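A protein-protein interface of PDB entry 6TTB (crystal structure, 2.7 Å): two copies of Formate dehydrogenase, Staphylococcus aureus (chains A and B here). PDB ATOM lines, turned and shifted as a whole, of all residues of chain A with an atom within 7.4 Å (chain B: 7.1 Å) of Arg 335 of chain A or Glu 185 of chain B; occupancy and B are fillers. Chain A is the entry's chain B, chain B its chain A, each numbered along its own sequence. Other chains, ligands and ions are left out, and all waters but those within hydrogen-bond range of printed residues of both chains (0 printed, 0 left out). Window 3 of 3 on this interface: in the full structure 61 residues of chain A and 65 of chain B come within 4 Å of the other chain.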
ATOM      1  N   LEU A  50       5.801  14.127   5.966  1.00  0.00           N
ATOM      2  CA  LEU A  50       4.628  14.747   5.344  1.00  0.00           C
ATOM      3  C   LEU A  50       3.940  13.846   4.274  1.00  0.00           C
ATOM      4  O   LEU A  50       2.701  13.688   4.288  1.00  0.00           O
ATOM      5  CB  LEU A  50       5.027  16.127   4.826  1.00  0.00           C
ATOM      6  CG  LEU A  50       5.167  17.186   5.918  1.00  0.00           C
ATOM      7  CD1 LEU A  50       5.797  18.452   5.365  1.00  0.00           C
ATOM      8  CD2 LEU A  50       3.777  17.528   6.555  1.00  0.00           C
ATOM      9  N   ILE A  57       0.376  15.719   3.153  1.00  0.00           N
ATOM     10  CA  ILE A  57       0.683  17.062   2.692  1.00  0.00           C
ATOM     11  C   ILE A  57      -0.531  17.982   2.844  1.00  0.00           C
ATOM     12  O   ILE A  57      -0.615  19.004   2.148  1.00  0.00           O
ATOM     13  CB  ILE A  57       1.256  17.088   1.247  1.00  0.00           C
ATOM     14  CG1 ILE A  57       0.390  16.304   0.238  1.00  0.00           C
ATOM     15  CG2 ILE A  57       2.750  16.674   1.188  1.00  0.00           C
ATOM     16  CD1 ILE A  57       1.042  16.117  -1.158  1.00  0.00           C
ATOM     17  N   VAL A 139       5.719  19.054  -9.421  1.00  0.00           N
ATOM     18  CA  VAL A 139       6.079  20.156  -8.563  1.00  0.00           C
ATOM     19  C   VAL A 139       7.567  20.269  -8.655  1.00  0.00           C
ATOM     20  O   VAL A 139       8.254  19.402  -8.124  1.00  0.00           O
ATOM     21  CB  VAL A 139       5.678  19.901  -7.107  1.00  0.00           C
ATOM     22  CG1 VAL A 139       6.072  21.090  -6.225  1.00  0.00           C
ATOM     23  CG2 VAL A 139       4.189  19.560  -6.958  1.00  0.00           C
ATOM     24  N   THR A 140       8.049  21.354  -9.272  1.00  0.00           N
ATOM     25  CA  THR A 140       9.477  21.483  -9.540  1.00  0.00           C
ATOM     26  C   THR A 140      10.230  21.918  -8.279  1.00  0.00           C
ATOM     27  O   THR A 140      11.053  22.825  -8.349  1.00  0.00           O
ATOM     28  CB  THR A 140       9.759  22.433 -10.720  1.00  0.00           C
ATOM     29  OG1 THR A 140       8.610  22.563 -11.561  1.00  0.00           O
ATOM     30  CG2 THR A 140      10.946  21.989 -11.549  1.00  0.00           C
ATOM     31  N   GLY A 141       9.959  21.246  -7.134  1.00  0.00           N
ATOM     32  CA  GLY A 141      10.638  21.524  -5.867  1.00  0.00           C
ATOM     33  C   GLY A 141      12.143  21.686  -6.071  1.00  0.00           C
ATOM     34  O   GLY A 141      12.753  20.916  -6.827  1.00  0.00           O
ATOM     35  N   SER A 142      12.725  22.749  -5.486  1.00  0.00           N
ATOM     36  CA  SER A 142      14.052  23.165  -5.939  1.00  0.00           C
ATOM     37  C   SER A 142      15.142  22.979  -4.867  1.00  0.00           C
ATOM     38  O   SER A 142      15.373  23.853  -4.023  1.00  0.00           O
ATOM     39  CB  SER A 142      14.088  24.537  -6.595  1.00  0.00           C
ATOM     40  OG  SER A 142      15.433  24.834  -6.978  1.00  0.00           O
ATOM     41  N   ASN A 143      15.916  21.896  -5.027  1.00  0.00           N
ATOM     42  CA  ASN A 143      16.849  21.456  -4.010  1.00  0.00           C
ATOM     43  C   ASN A 143      18.271  21.770  -4.449  1.00  0.00           C
ATOM     44  O   ASN A 143      19.181  21.030  -4.143  1.00  0.00           O
ATOM     45  CB  ASN A 143      16.695  19.956  -3.723  1.00  0.00           C
ATOM     46  CG  ASN A 143      15.243  19.479  -3.781  1.00  0.00           C
ATOM     47  OD1 ASN A 143      14.433  19.859  -2.945  1.00  0.00           O
ATOM     48  ND2 ASN A 143      14.885  18.694  -4.798  1.00  0.00           N
ATOM     49  N   THR A 144      18.475  22.857  -5.173  1.00  0.00           N
ATOM     50  CA  THR A 144      19.850  23.167  -5.471  1.00  0.00           C
ATOM     51  C   THR A 144      20.662  23.290  -4.180  1.00  0.00           C
ATOM     52  O   THR A 144      21.707  22.685  -4.063  1.00  0.00           O
ATOM     53  CB  THR A 144      19.991  24.320  -6.469  1.00  0.00           C
ATOM     54  OG1 THR A 144      19.137  25.390  -6.058  1.00  0.00           O
ATOM     55  CG2 THR A 144      19.681  23.885  -7.872  1.00  0.00           C
ATOM     56  N   VAL A 145      20.162  24.047  -3.211  1.00  0.00           N
ATOM     57  CA  VAL A 145      20.908  24.360  -1.988  1.00  0.00           C
ATOM     58  C   VAL A 145      21.135  23.101  -1.206  1.00  0.00           C
ATOM     59  O   VAL A 145      22.240  22.866  -0.727  1.00  0.00           O
ATOM     60  CB  VAL A 145      20.155  25.361  -1.095  1.00  0.00           C
ATOM     61  CG1 VAL A 145      20.724  25.385   0.315  1.00  0.00           C
ATOM     62  CG2 VAL A 145      20.170  26.759  -1.709  1.00  0.00           C
ATOM     63  N   SER A 146      20.078  22.300  -1.086  1.00  0.00           N
ATOM     64  CA  SER A 146      20.183  20.992  -0.451  1.00  0.00           C
ATOM     65  C   SER A 146      21.368  20.274  -1.003  1.00  0.00           C
ATOM     66  O   SER A 146      22.188  19.776  -0.247  1.00  0.00           O
ATOM     67  CB  SER A 146      18.962  20.147  -0.659  1.00  0.00           C
ATOM     68  OG  SER A 146      18.991  18.957   0.134  1.00  0.00           O
ATOM     69  N   VAL A 147      21.432  20.173  -2.320  1.00  0.00           N
ATOM     70  CA  VAL A 147      22.433  19.297  -2.901  1.00  0.00           C
ATOM     71  C   VAL A 147      23.804  19.885  -2.580  1.00  0.00           C
ATOM     72  O   VAL A 147      24.785  19.161  -2.275  1.00  0.00           O
ATOM     73  CB  VAL A 147      22.173  19.034  -4.402  1.00  0.00           C
ATOM     74  CG1 VAL A 147      23.291  18.244  -5.054  1.00  0.00           C
ATOM     75  CG2 VAL A 147      20.863  18.296  -4.601  1.00  0.00           C
ATOM     76  N   GLU A 149      24.706  21.586   0.069  1.00  0.00           N
ATOM     77  CA  GLU A 149      25.026  21.266   1.462  1.00  0.00           C
ATOM     78  C   GLU A 149      25.498  19.825   1.533  1.00  0.00           C
ATOM     79  O   GLU A 149      26.524  19.526   2.111  1.00  0.00           O
ATOM     80  CB  GLU A 149      23.779  21.341   2.326  1.00  0.00           C
ATOM     81  CG  GLU A 149      23.194  22.724   2.440  1.00  0.00           C
ATOM     82  CD  GLU A 149      21.982  22.770   3.342  1.00  0.00           C
ATOM     83  OE1 GLU A 149      21.438  21.618   3.724  1.00  0.00           O
ATOM     84  OE2 GLU A 149      21.551  23.924   3.684  1.00  0.00           O
ATOM     85  N   SER A 326      16.931  13.952  -0.348  1.00  0.00           N
ATOM     86  CA  SER A 326      17.546  15.261  -0.549  1.00  0.00           C
ATOM     87  C   SER A 326      16.573  16.077  -1.333  1.00  0.00           C
ATOM     88  O   SER A 326      16.257  17.206  -0.962  1.00  0.00           O
ATOM     89  CB  SER A 326      18.876  15.209  -1.285  1.00  0.00           C
ATOM     90  N   THR A 329      14.131  16.101   2.026  1.00  0.00           N
ATOM     91  CA  THR A 329      14.238  16.801   3.298  1.00  0.00           C
ATOM     92  C   THR A 329      12.857  17.296   3.679  1.00  0.00           C
ATOM     93  O   THR A 329      11.963  17.434   2.825  1.00  0.00           O
ATOM     94  CB  THR A 329      15.118  18.047   3.192  1.00  0.00           C
ATOM     95  OG1 THR A 329      14.401  18.992   2.398  1.00  0.00           O
ATOM     96  CG2 THR A 329      16.471  17.783   2.568  1.00  0.00           C
ATOM     97  N   LEU A 330      12.688  17.575   4.972  1.00  0.00           N
ATOM     98  CA  LEU A 330      11.407  18.004   5.485  1.00  0.00           C
ATOM     99  C   LEU A 330      10.877  19.231   4.713  1.00  0.00           C
ATOM    100  O   LEU A 330       9.717  19.287   4.346  1.00  0.00           O
ATOM    101  CB  LEU A 330      11.542  18.236   6.990  1.00  0.00           C
ATOM    102  CG  LEU A 330      10.749  17.260   7.892  1.00  0.00           C
ATOM    103  CD1 LEU A 330      10.158  16.044   7.131  1.00  0.00           C
ATOM    104  CD2 LEU A 330      11.557  16.844   9.123  1.00  0.00           C
ATOM    105  N   GLU A 331      11.738  20.191   4.400  1.00  0.00           N
ATOM    106  CA  GLU A 331      11.260  21.376   3.726  1.00  0.00           C
ATOM    107  C   GLU A 331      11.225  21.141   2.209  1.00  0.00           C
ATOM    108  O   GLU A 331      10.622  21.901   1.445  1.00  0.00           O
ATOM    109  CB  GLU A 331      12.067  22.588   4.169  1.00  0.00           C
ATOM    110  CG  GLU A 331      13.553  22.378   4.140  1.00  0.00           C
ATOM    111  CD  GLU A 331      14.114  21.693   5.391  1.00  0.00           C
ATOM    112  OE1 GLU A 331      14.338  20.478   5.335  1.00  0.00           O
ATOM    113  OE2 GLU A 331      14.328  22.371   6.412  1.00  0.00           O
ATOM    114  N   ALA A 332      11.852  20.075   1.748  1.00  0.00           N
ATOM    115  CA  ALA A 332      11.502  19.657   0.412  1.00  0.00           C
ATOM    116  C   ALA A 332      10.046  19.192   0.408  1.00  0.00           C
ATOM    117  O   ALA A 332       9.304  19.518  -0.492  1.00  0.00           O
ATOM    118  CB  ALA A 332      12.465  18.613  -0.095  1.00  0.00           C
ATOM    119  N   GLN A 333       9.628  18.485   1.455  1.00  0.00           N
ATOM    120  CA  GLN A 333       8.205  18.139   1.601  1.00  0.00           C
ATOM    121  C   GLN A 333       7.335  19.399   1.737  1.00  0.00           C
ATOM    122  O   GLN A 333       6.371  19.511   1.013  1.00  0.00           O
ATOM    123  CB  GLN A 333       7.954  17.071   2.665  1.00  0.00           C
ATOM    124  CG  GLN A 333       8.723  15.783   2.396  1.00  0.00           C
ATOM    125  CD  GLN A 333       8.779  14.877   3.594  1.00  0.00           C
ATOM    126  OE1 GLN A 333       7.753  14.571   4.193  1.00  0.00           O
ATOM    127  NE2 GLN A 333       9.985  14.420   3.935  1.00  0.00           N
ATOM    128  N   LYS A 334       7.721  20.394   2.576  1.00  0.00           N
ATOM    129  CA  LYS A 334       6.850  21.558   2.659  1.00  0.00           C
ATOM    130  C   LYS A 334       6.704  22.169   1.271  1.00  0.00           C
ATOM    131  O   LYS A 334       5.592  22.478   0.861  1.00  0.00           O
ATOM    132  CB  LYS A 334       7.131  22.536   3.825  1.00  0.00           C
ATOM    133  N   ARG A 335       7.806  22.193   0.506  1.00  0.00           N
ATOM    134  CA  ARG A 335       7.775  22.740  -0.831  1.00  0.00           C
ATOM    135  C   ARG A 335       6.739  22.017  -1.666  1.00  0.00           C
ATOM    136  O   ARG A 335       5.802  22.643  -2.163  1.00  0.00           O
ATOM    137  CB  ARG A 335       9.153  22.802  -1.445  1.00  0.00           C
ATOM    138  CG  ARG A 335       9.885  24.076  -1.037  1.00  0.00           C
ATOM    139  CD  ARG A 335      11.106  24.265  -1.901  1.00  0.00           C
ATOM    140  NE  ARG A 335      12.240  23.485  -1.415  1.00  0.00           N
ATOM    141  CZ  ARG A 335      13.058  23.878  -0.442  1.00  0.00           C
ATOM    142  NH1 ARG A 335      12.845  25.020   0.201  1.00  0.00           N
ATOM    143  NH2 ARG A 335      14.093  23.129  -0.114  1.00  0.00           N
ATOM    144  N   ILE A 336       6.794  20.682  -1.659  1.00  0.00           N
ATOM    145  CA  ILE A 336       5.857  19.876  -2.425  1.00  0.00           C
ATOM    146  C   ILE A 336       4.430  20.132  -1.951  1.00  0.00           C
ATOM    147  O   ILE A 336       3.542  20.381  -2.757  1.00  0.00           O
ATOM    148  CB  ILE A 336       6.213  18.384  -2.374  1.00  0.00           C
ATOM    149  CG1 ILE A 336       7.483  18.088  -3.176  1.00  0.00           C
ATOM    150  CG2 ILE A 336       5.029  17.564  -2.882  1.00  0.00           C
ATOM    151  CD1 ILE A 336       7.756  16.640  -3.354  1.00  0.00           C
ATOM    152  N   GLU A 337       4.219  20.024  -0.651  1.00  0.00           N
ATOM    153  CA  GLU A 337       2.955  20.358  -0.026  1.00  0.00           C
ATOM    154  C   GLU A 337       2.371  21.610  -0.670  1.00  0.00           C
ATOM    155  O   GLU A 337       1.256  21.593  -1.190  1.00  0.00           O
ATOM    156  CB  GLU A 337       3.185  20.700   1.441  1.00  0.00           C
ATOM    157  CG  GLU A 337       1.908  21.221   2.062  1.00  0.00           C
ATOM    158  CD  GLU A 337       1.613  20.954   3.521  1.00  0.00           C
ATOM    159  OE1 GLU A 337       2.197  19.989   4.115  1.00  0.00           O
ATOM    160  OE2 GLU A 337       0.692  21.596   4.014  1.00  0.00           O
ATOM    161  N   ASP A 338       3.143  22.698  -0.610  1.00  0.00           N
ATOM    162  CA  ASP A 338       2.663  24.004  -1.051  1.00  0.00           C
ATOM    163  C   ASP A 338       2.322  23.998  -2.535  1.00  0.00           C
ATOM    164  O   ASP A 338       1.389  24.671  -2.932  1.00  0.00           O
ATOM    165  CB  ASP A 338       3.707  25.095  -0.836  1.00  0.00           C
ATOM    166  CG  ASP A 338       3.929  25.414   0.608  1.00  0.00           C
ATOM    167  OD1 ASP A 338       3.068  25.003   1.456  1.00  0.00           O
ATOM    168  OD2 ASP A 338       4.972  26.017   0.894  1.00  0.00           O
ATOM    169  N   GLY A 339       3.190  23.353  -3.328  1.00  0.00           N
ATOM    170  CA  GLY A 339       3.024  23.189  -4.752  1.00  0.00           C
ATOM    171  C   GLY A 339       1.780  22.368  -5.099  1.00  0.00           C
ATOM    172  O   GLY A 339       1.006  22.777  -5.944  1.00  0.00           O
ATOM    173  N   VAL A 340       1.611  21.176  -4.498  1.00  0.00           N
ATOM    174  CA  VAL A 340       0.445  20.399  -4.848  1.00  0.00           C
ATOM    175  C   VAL A 340      -0.783  21.262  -4.577  1.00  0.00           C
ATOM    176  O   VAL A 340      -1.732  21.257  -5.342  1.00  0.00           O
ATOM    177  CB  VAL A 340       0.391  19.064  -4.098  1.00  0.00           C
ATOM    178  CG1 VAL A 340      -0.907  18.321  -4.360  1.00  0.00           C
ATOM    179  CG2 VAL A 340       1.553  18.191  -4.460  1.00  0.00           C
ATOM    180  N   LYS A 341      -0.736  22.023  -3.486  1.00  0.00           N
ATOM    181  CA  LYS A 341      -1.805  22.919  -3.114  1.00  0.00           C
ATOM    182  C   LYS A 341      -1.920  23.986  -4.169  1.00  0.00           C
ATOM    183  O   LYS A 341      -3.013  24.260  -4.613  1.00  0.00           O
ATOM    184  CB  LYS A 341      -1.551  23.581  -1.747  1.00  0.00           C
ATOM    185  CG  LYS A 341      -1.523  22.656  -0.517  1.00  0.00           C
ATOM    186  CD  LYS A 341      -2.018  23.252   0.717  1.00  0.00           C
ATOM    187  CE  LYS A 341      -1.604  22.430   1.885  1.00  0.00           C
ATOM    188  NZ  LYS A 341      -1.249  23.324   3.026  1.00  0.00           N
ATOM    189  N   ASP A 342      -0.820  24.666  -4.491  1.00  0.00           N
ATOM    190  CA  ASP A 342      -0.910  25.757  -5.462  1.00  0.00           C
ATOM    191  C   ASP A 342      -1.484  25.257  -6.829  1.00  0.00           C
ATOM    192  O   ASP A 342      -2.297  25.944  -7.449  1.00  0.00           O
ATOM    193  CB  ASP A 342       0.341  26.637  -5.503  1.00  0.00           C
ATOM    194  CG  ASP A 342       0.393  27.560  -6.724  1.00  0.00           C
ATOM    195  OD1 ASP A 342      -0.248  28.581  -6.709  1.00  0.00           O
ATOM    196  OD2 ASP A 342       1.051  27.202  -7.705  1.00  0.00           O
ATOM    197  N   LEU B 156      25.839  19.716   9.846  1.00  0.00           N
ATOM    198  CA  LEU B 156      25.359  19.141   8.623  1.00  0.00           C
ATOM    199  C   LEU B 156      24.932  17.696   8.851  1.00  0.00           C
ATOM    200  O   LEU B 156      23.826  17.352   8.541  1.00  0.00           O
ATOM    201  CB  LEU B 156      26.462  19.273   7.570  1.00  0.00           C
ATOM    202  CG  LEU B 156      26.687  20.701   7.044  1.00  0.00           C
ATOM    203  CD1 LEU B 156      28.029  20.839   6.370  1.00  0.00           C
ATOM    204  CD2 LEU B 156      25.595  21.118   6.078  1.00  0.00           C
ATOM    205  N   LEU B 159      21.611  17.719  10.880  1.00  0.00           N
ATOM    206  CA  LEU B 159      20.372  18.194  10.255  1.00  0.00           C
ATOM    207  C   LEU B 159      20.040  17.334   9.043  1.00  0.00           C
ATOM    208  O   LEU B 159      18.902  17.039   8.769  1.00  0.00           O
ATOM    209  CB  LEU B 159      20.484  19.675   9.859  1.00  0.00           C
ATOM    210  CG  LEU B 159      20.273  20.650  11.021  1.00  0.00           C
ATOM    211  CD1 LEU B 159      21.285  21.765  10.926  1.00  0.00           C
ATOM    212  CD2 LEU B 159      18.850  21.203  11.077  1.00  0.00           C
ATOM    213  N   ARG B 160      21.055  16.897   8.338  1.00  0.00           N
ATOM    214  CA  ARG B 160      20.781  16.231   7.088  1.00  0.00           C
ATOM    215  C   ARG B 160      20.495  14.770   7.366  1.00  0.00           C
ATOM    216  O   ARG B 160      20.057  14.043   6.470  1.00  0.00           O
ATOM    217  CB  ARG B 160      21.898  16.489   6.068  1.00  0.00           C
ATOM    218  CG  ARG B 160      21.909  17.922   5.581  1.00  0.00           C
ATOM    219  CD  ARG B 160      22.610  18.102   4.267  1.00  0.00           C
ATOM    220  NE  ARG B 160      21.982  17.415   3.158  1.00  0.00           N
ATOM    221  CZ  ARG B 160      21.073  17.975   2.392  1.00  0.00           C
ATOM    222  NH1 ARG B 160      20.630  19.202   2.679  1.00  0.00           N
ATOM    223  NH2 ARG B 160      20.607  17.310   1.340  1.00  0.00           N
ATOM    224  N   ALA B 183      15.276  14.592   8.063  1.00  0.00           N
ATOM    225  CA  ALA B 183      16.220  15.241   7.190  1.00  0.00           C
ATOM    226  C   ALA B 183      15.730  16.654   6.886  1.00  0.00           C
ATOM    227  O   ALA B 183      14.570  16.884   6.555  1.00  0.00           O
ATOM    228  CB  ALA B 183      16.349  14.430   5.947  1.00  0.00           C
ATOM    229  N   HIS B 184      16.620  17.597   7.106  1.00  0.00           N
ATOM    230  CA  HIS B 184      16.388  19.017   7.067  1.00  0.00           C
ATOM    231  C   HIS B 184      17.515  19.602   6.251  1.00  0.00           C
ATOM    232  O   HIS B 184      18.599  19.050   6.239  1.00  0.00           O
ATOM    233  CB  HIS B 184      16.506  19.615   8.470  1.00  0.00           C
ATOM    234  CG  HIS B 184      15.342  19.308   9.367  1.00  0.00           C
ATOM    235  ND1 HIS B 184      14.246  20.184   9.520  1.00  0.00           N
ATOM    236  CD2 HIS B 184      15.073  18.248  10.163  1.00  0.00           C
ATOM    237  CE1 HIS B 184      13.396  19.659  10.377  1.00  0.00           C
ATOM    238  NE2 HIS B 184      13.845  18.483  10.745  1.00  0.00           N
ATOM    239  N   GLU B 185      17.208  20.641   5.492  1.00  0.00           N
ATOM    240  CA  GLU B 185      18.207  21.549   5.008  1.00  0.00           C
ATOM    241  C   GLU B 185      18.783  22.318   6.188  1.00  0.00           C
ATOM    242  O   GLU B 185      18.050  22.742   7.078  1.00  0.00           O
ATOM    243  CB  GLU B 185      17.519  22.515   4.063  1.00  0.00           C
ATOM    244  CG  GLU B 185      16.840  21.795   2.939  1.00  0.00           C
ATOM    245  CD  GLU B 185      16.612  22.674   1.742  1.00  0.00           C
ATOM    246  OE1 GLU B 185      16.950  22.225   0.646  1.00  0.00           O
ATOM    247  OE2 GLU B 185      16.118  23.818   1.921  1.00  0.00           O
ATOM    248  N   LEU B 186      20.073  22.589   6.133  1.00  0.00           N
ATOM    249  CA  LEU B 186      20.647  23.482   7.100  1.00  0.00           C
ATOM    250  C   LEU B 186      20.168  24.913   6.814  1.00  0.00           C
ATOM    251  O   LEU B 186      20.090  25.779   7.714  1.00  0.00           O
ATOM    252  CB  LEU B 186      22.159  23.374   6.999  1.00  0.00           C
ATOM    253  CG  LEU B 186      22.877  24.386   7.869  1.00  0.00           C
ATOM    254  CD1 LEU B 186      22.481  24.165   9.326  1.00  0.00           C
ATOM    255  CD2 LEU B 186      24.379  24.315   7.699  1.00  0.00           C
ATOM    256  N   GLN B 187      19.915  25.194   5.538  1.00  0.00           N
ATOM    257  CA  GLN B 187      19.597  26.563   5.157  1.00  0.00           C
ATOM    258  C   GLN B 187      18.296  27.033   5.870  1.00  0.00           C
ATOM    259  O   GLN B 187      17.372  26.250   6.099  1.00  0.00           O
ATOM    260  CB  GLN B 187      19.511  26.614   3.654  1.00  0.00           C
ATOM    261  CG  GLN B 187      18.881  27.869   3.123  1.00  0.00           C
ATOM    262  CD  GLN B 187      18.374  27.625   1.725  1.00  0.00           C
ATOM    263  OE1 GLN B 187      18.568  28.437   0.851  1.00  0.00           O
ATOM    264  NE2 GLN B 187      17.808  26.448   1.489  1.00  0.00           N
ATOM    265  N   HIS B 188      18.274  28.322   6.248  1.00  0.00           N
ATOM    266  CA  HIS B 188      17.144  28.993   6.883  1.00  0.00           C
ATOM    267  C   HIS B 188      17.014  28.640   8.370  1.00  0.00           C
ATOM    268  O   HIS B 188      16.148  29.159   9.030  1.00  0.00           O
ATOM    269  CB  HIS B 188      15.823  28.785   6.095  1.00  0.00           C
ATOM    270  CG  HIS B 188      15.775  29.402   4.718  1.00  0.00           C
ATOM    271  ND1 HIS B 188      15.983  30.777   4.482  1.00  0.00           N
ATOM    272  CD2 HIS B 188      15.634  28.842   3.503  1.00  0.00           C
ATOM    273  CE1 HIS B 188      15.934  31.021   3.179  1.00  0.00           C
ATOM    274  NE2 HIS B 188      15.775  29.842   2.554  1.00  0.00           N
ATOM    275  N   LYS B 189      17.889  27.779   8.908  1.00  0.00           N
ATOM    276  CA  LYS B 189      17.807  27.441  10.312  1.00  0.00           C
ATOM    277  C   LYS B 189      18.503  28.524  11.126  1.00  0.00           C
ATOM    278  O   LYS B 189      19.394  29.243  10.609  1.00  0.00           O
ATOM    279  CB  LYS B 189      18.481  26.100  10.584  1.00  0.00           C
ATOM    280  CG  LYS B 189      17.966  24.917   9.763  1.00  0.00           C
ATOM    281  CD  LYS B 189      16.937  24.109  10.487  1.00  0.00           C
ATOM    282  CE  LYS B 189      16.053  23.319   9.547  1.00  0.00           C
ATOM    283  NZ  LYS B 189      15.945  24.043   8.270  1.00  0.00           N
ATOM    284  N   VAL B 212      21.324  31.182   6.838  1.00  0.00           N
ATOM    285  CA  VAL B 212      21.104  30.628   8.145  1.00  0.00           C
ATOM    286  C   VAL B 212      21.178  31.860   9.046  1.00  0.00           C
ATOM    287  O   VAL B 212      21.942  32.751   8.746  1.00  0.00           O
ATOM    288  CB  VAL B 212      22.234  29.568   8.420  1.00  0.00           C
ATOM    289  CG1 VAL B 212      23.260  29.973   9.449  1.00  0.00           C
ATOM    290  CG2 VAL B 212      21.715  28.155   8.656  1.00  0.00           C
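No position is printed for both chains.
Glu 185 of chain B touches just these residues of chain A: Ser 146, Glu 149, Thr 329, Glu 331 and Arg 335.
Of the printed residues of chain B, Val 145 of chain A touches Gln 187 (3.3 Å).
Printed residues of chain A within 4 Å of Leu 186 of chain B: Glu 149.
Leu 159 of chain B touches none of the printed residues of chain A.
Asp 338 of chain A touches none of the printed residues of chain B.
The nearest residue of chain B that does not touch Arg 335 of chain A is Gln 187 of chain B (5.2 Å).
The nearest residue of chain A that does not touch Glu 185 of chain B is Val 145 of chain A (4.7 Å).
Printed residues of chain B that touch a printed residue of chain A: Arg 160, Ala 183, His 184, Glu 185, Leu 186, Gln 187 and Lys 189.
Hydrophobic or aromatic side chains of chain B that line the printed part of chain A: His 184 and Leu 186.
Along chain B the printed residues that touch a printed residue of chain A span positions 160 to 189.
Hydrophobic or aromatic side chains of chain A that line the printed part of chain B: Val 145 and Leu 330.
Among the printed residues, 17 pairs touch across the chains.
Among the printed residues, Asp or Glu carboxylates within 4 Å of a Lys or Arg side-chain nitrogen of the other chain: Glu 149 of chain A with Arg 160 of chain B (2.8 Å), Glu 331 of chain A with Lys 189 of chain B (3.0 Å) and Arg 335 of chain A with Glu 185 of chain B (3.0 Å).
OG of Ser 146 of chain A lies within hydrogen-bond range of NH2 of Arg 160 of chain B, at 2.6 Å.
The guanidinium group (NH1) of Arg 160 of chain B lies within salt-bridge range of the side-chain carboxylate (OE1) of Glu 149 of chain A (2.8 Å).
N of Leu 330 of chain A lies within hydrogen-bond range of O of Ala 183 of chain B (2.6 Å).
N of Glu 185 of chain B is in hydrogen-bond range of OE1 of Glu 331 of chain A (2.9 Å).
OE2 of Glu 185 of chain B lies within salt-bridge range of NH2 of Arg 335 of chain A, at 3.0 Å.
The backbone NH (N) of Leu 186 of chain B sits at hydrogen-bond distance from the side-chain carboxylate (OE1) of Glu 149 of chain A.
N of Gln 187 of chain B lies within hydrogen-bond range of OE2 of Glu 149 of chain A (2.8 Å).
The side-chain carboxylate (OE2) of Glu 331 of chain A lies within salt-bridge range of the side-chain amino group (NZ) of Lys 189 of chain B.
Gln 187 of chain B touches Val 145 of chain A.
CB of Ser 146 of chain A touches OE1 of Glu 185 of chain B, at 3.2 Å.
Glu 185 of chain B touches Glu 149 of chain A (CA to OE1, 3.5 Å).
NH2 of Arg 160 of chain B touches CB of Ser 326 of chain A (3.8 Å).
CA of Thr 329 of chain A touches O of Ala 183 of chain B (3.3 Å).
CG of Glu 185 of chain B touches OG1 of Thr 329 of chain A, at 3.8 Å.
His 184 of chain B touches Leu 330 of chain A.
Glu 331 of chain A touches Ala 183 of chain B (OE1 to O, 3.8 Å).
His 184 of chain B touches Glu 331 of chain A (CA to OE1, 3.1 Å).
The backbone carbonyl oxygen (O) of Leu 159 of chain B is in hydrogen-bond range of the backbone NH (N) of His 184 of chain B (2.9 Å).
The backbone carbonyl oxygen of Glu 185 of chain B lies within hydrogen-bond range of the side-chain amino group of Lys 189 of chain B, 2.7 Å away.
O of Gln 187 of chain B lies within hydrogen-bond range of NZ of Lys 189 of chain B (3.4 Å).
OG of Ser 146 of chain A sits at hydrogen-bond distance from O of Ser 326 of chain A, at 3.4 Å.
The side-chain hydroxyl of Thr 329 of chain A lies within hydrogen-bond range of the side-chain carboxylate of Glu 331 of chain A (3.3 Å).
The side-chain hydroxyl of Thr 329 of chain A is in hydrogen-bond range of the backbone NH of Ala 332 of chain A, at 2.8 Å.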
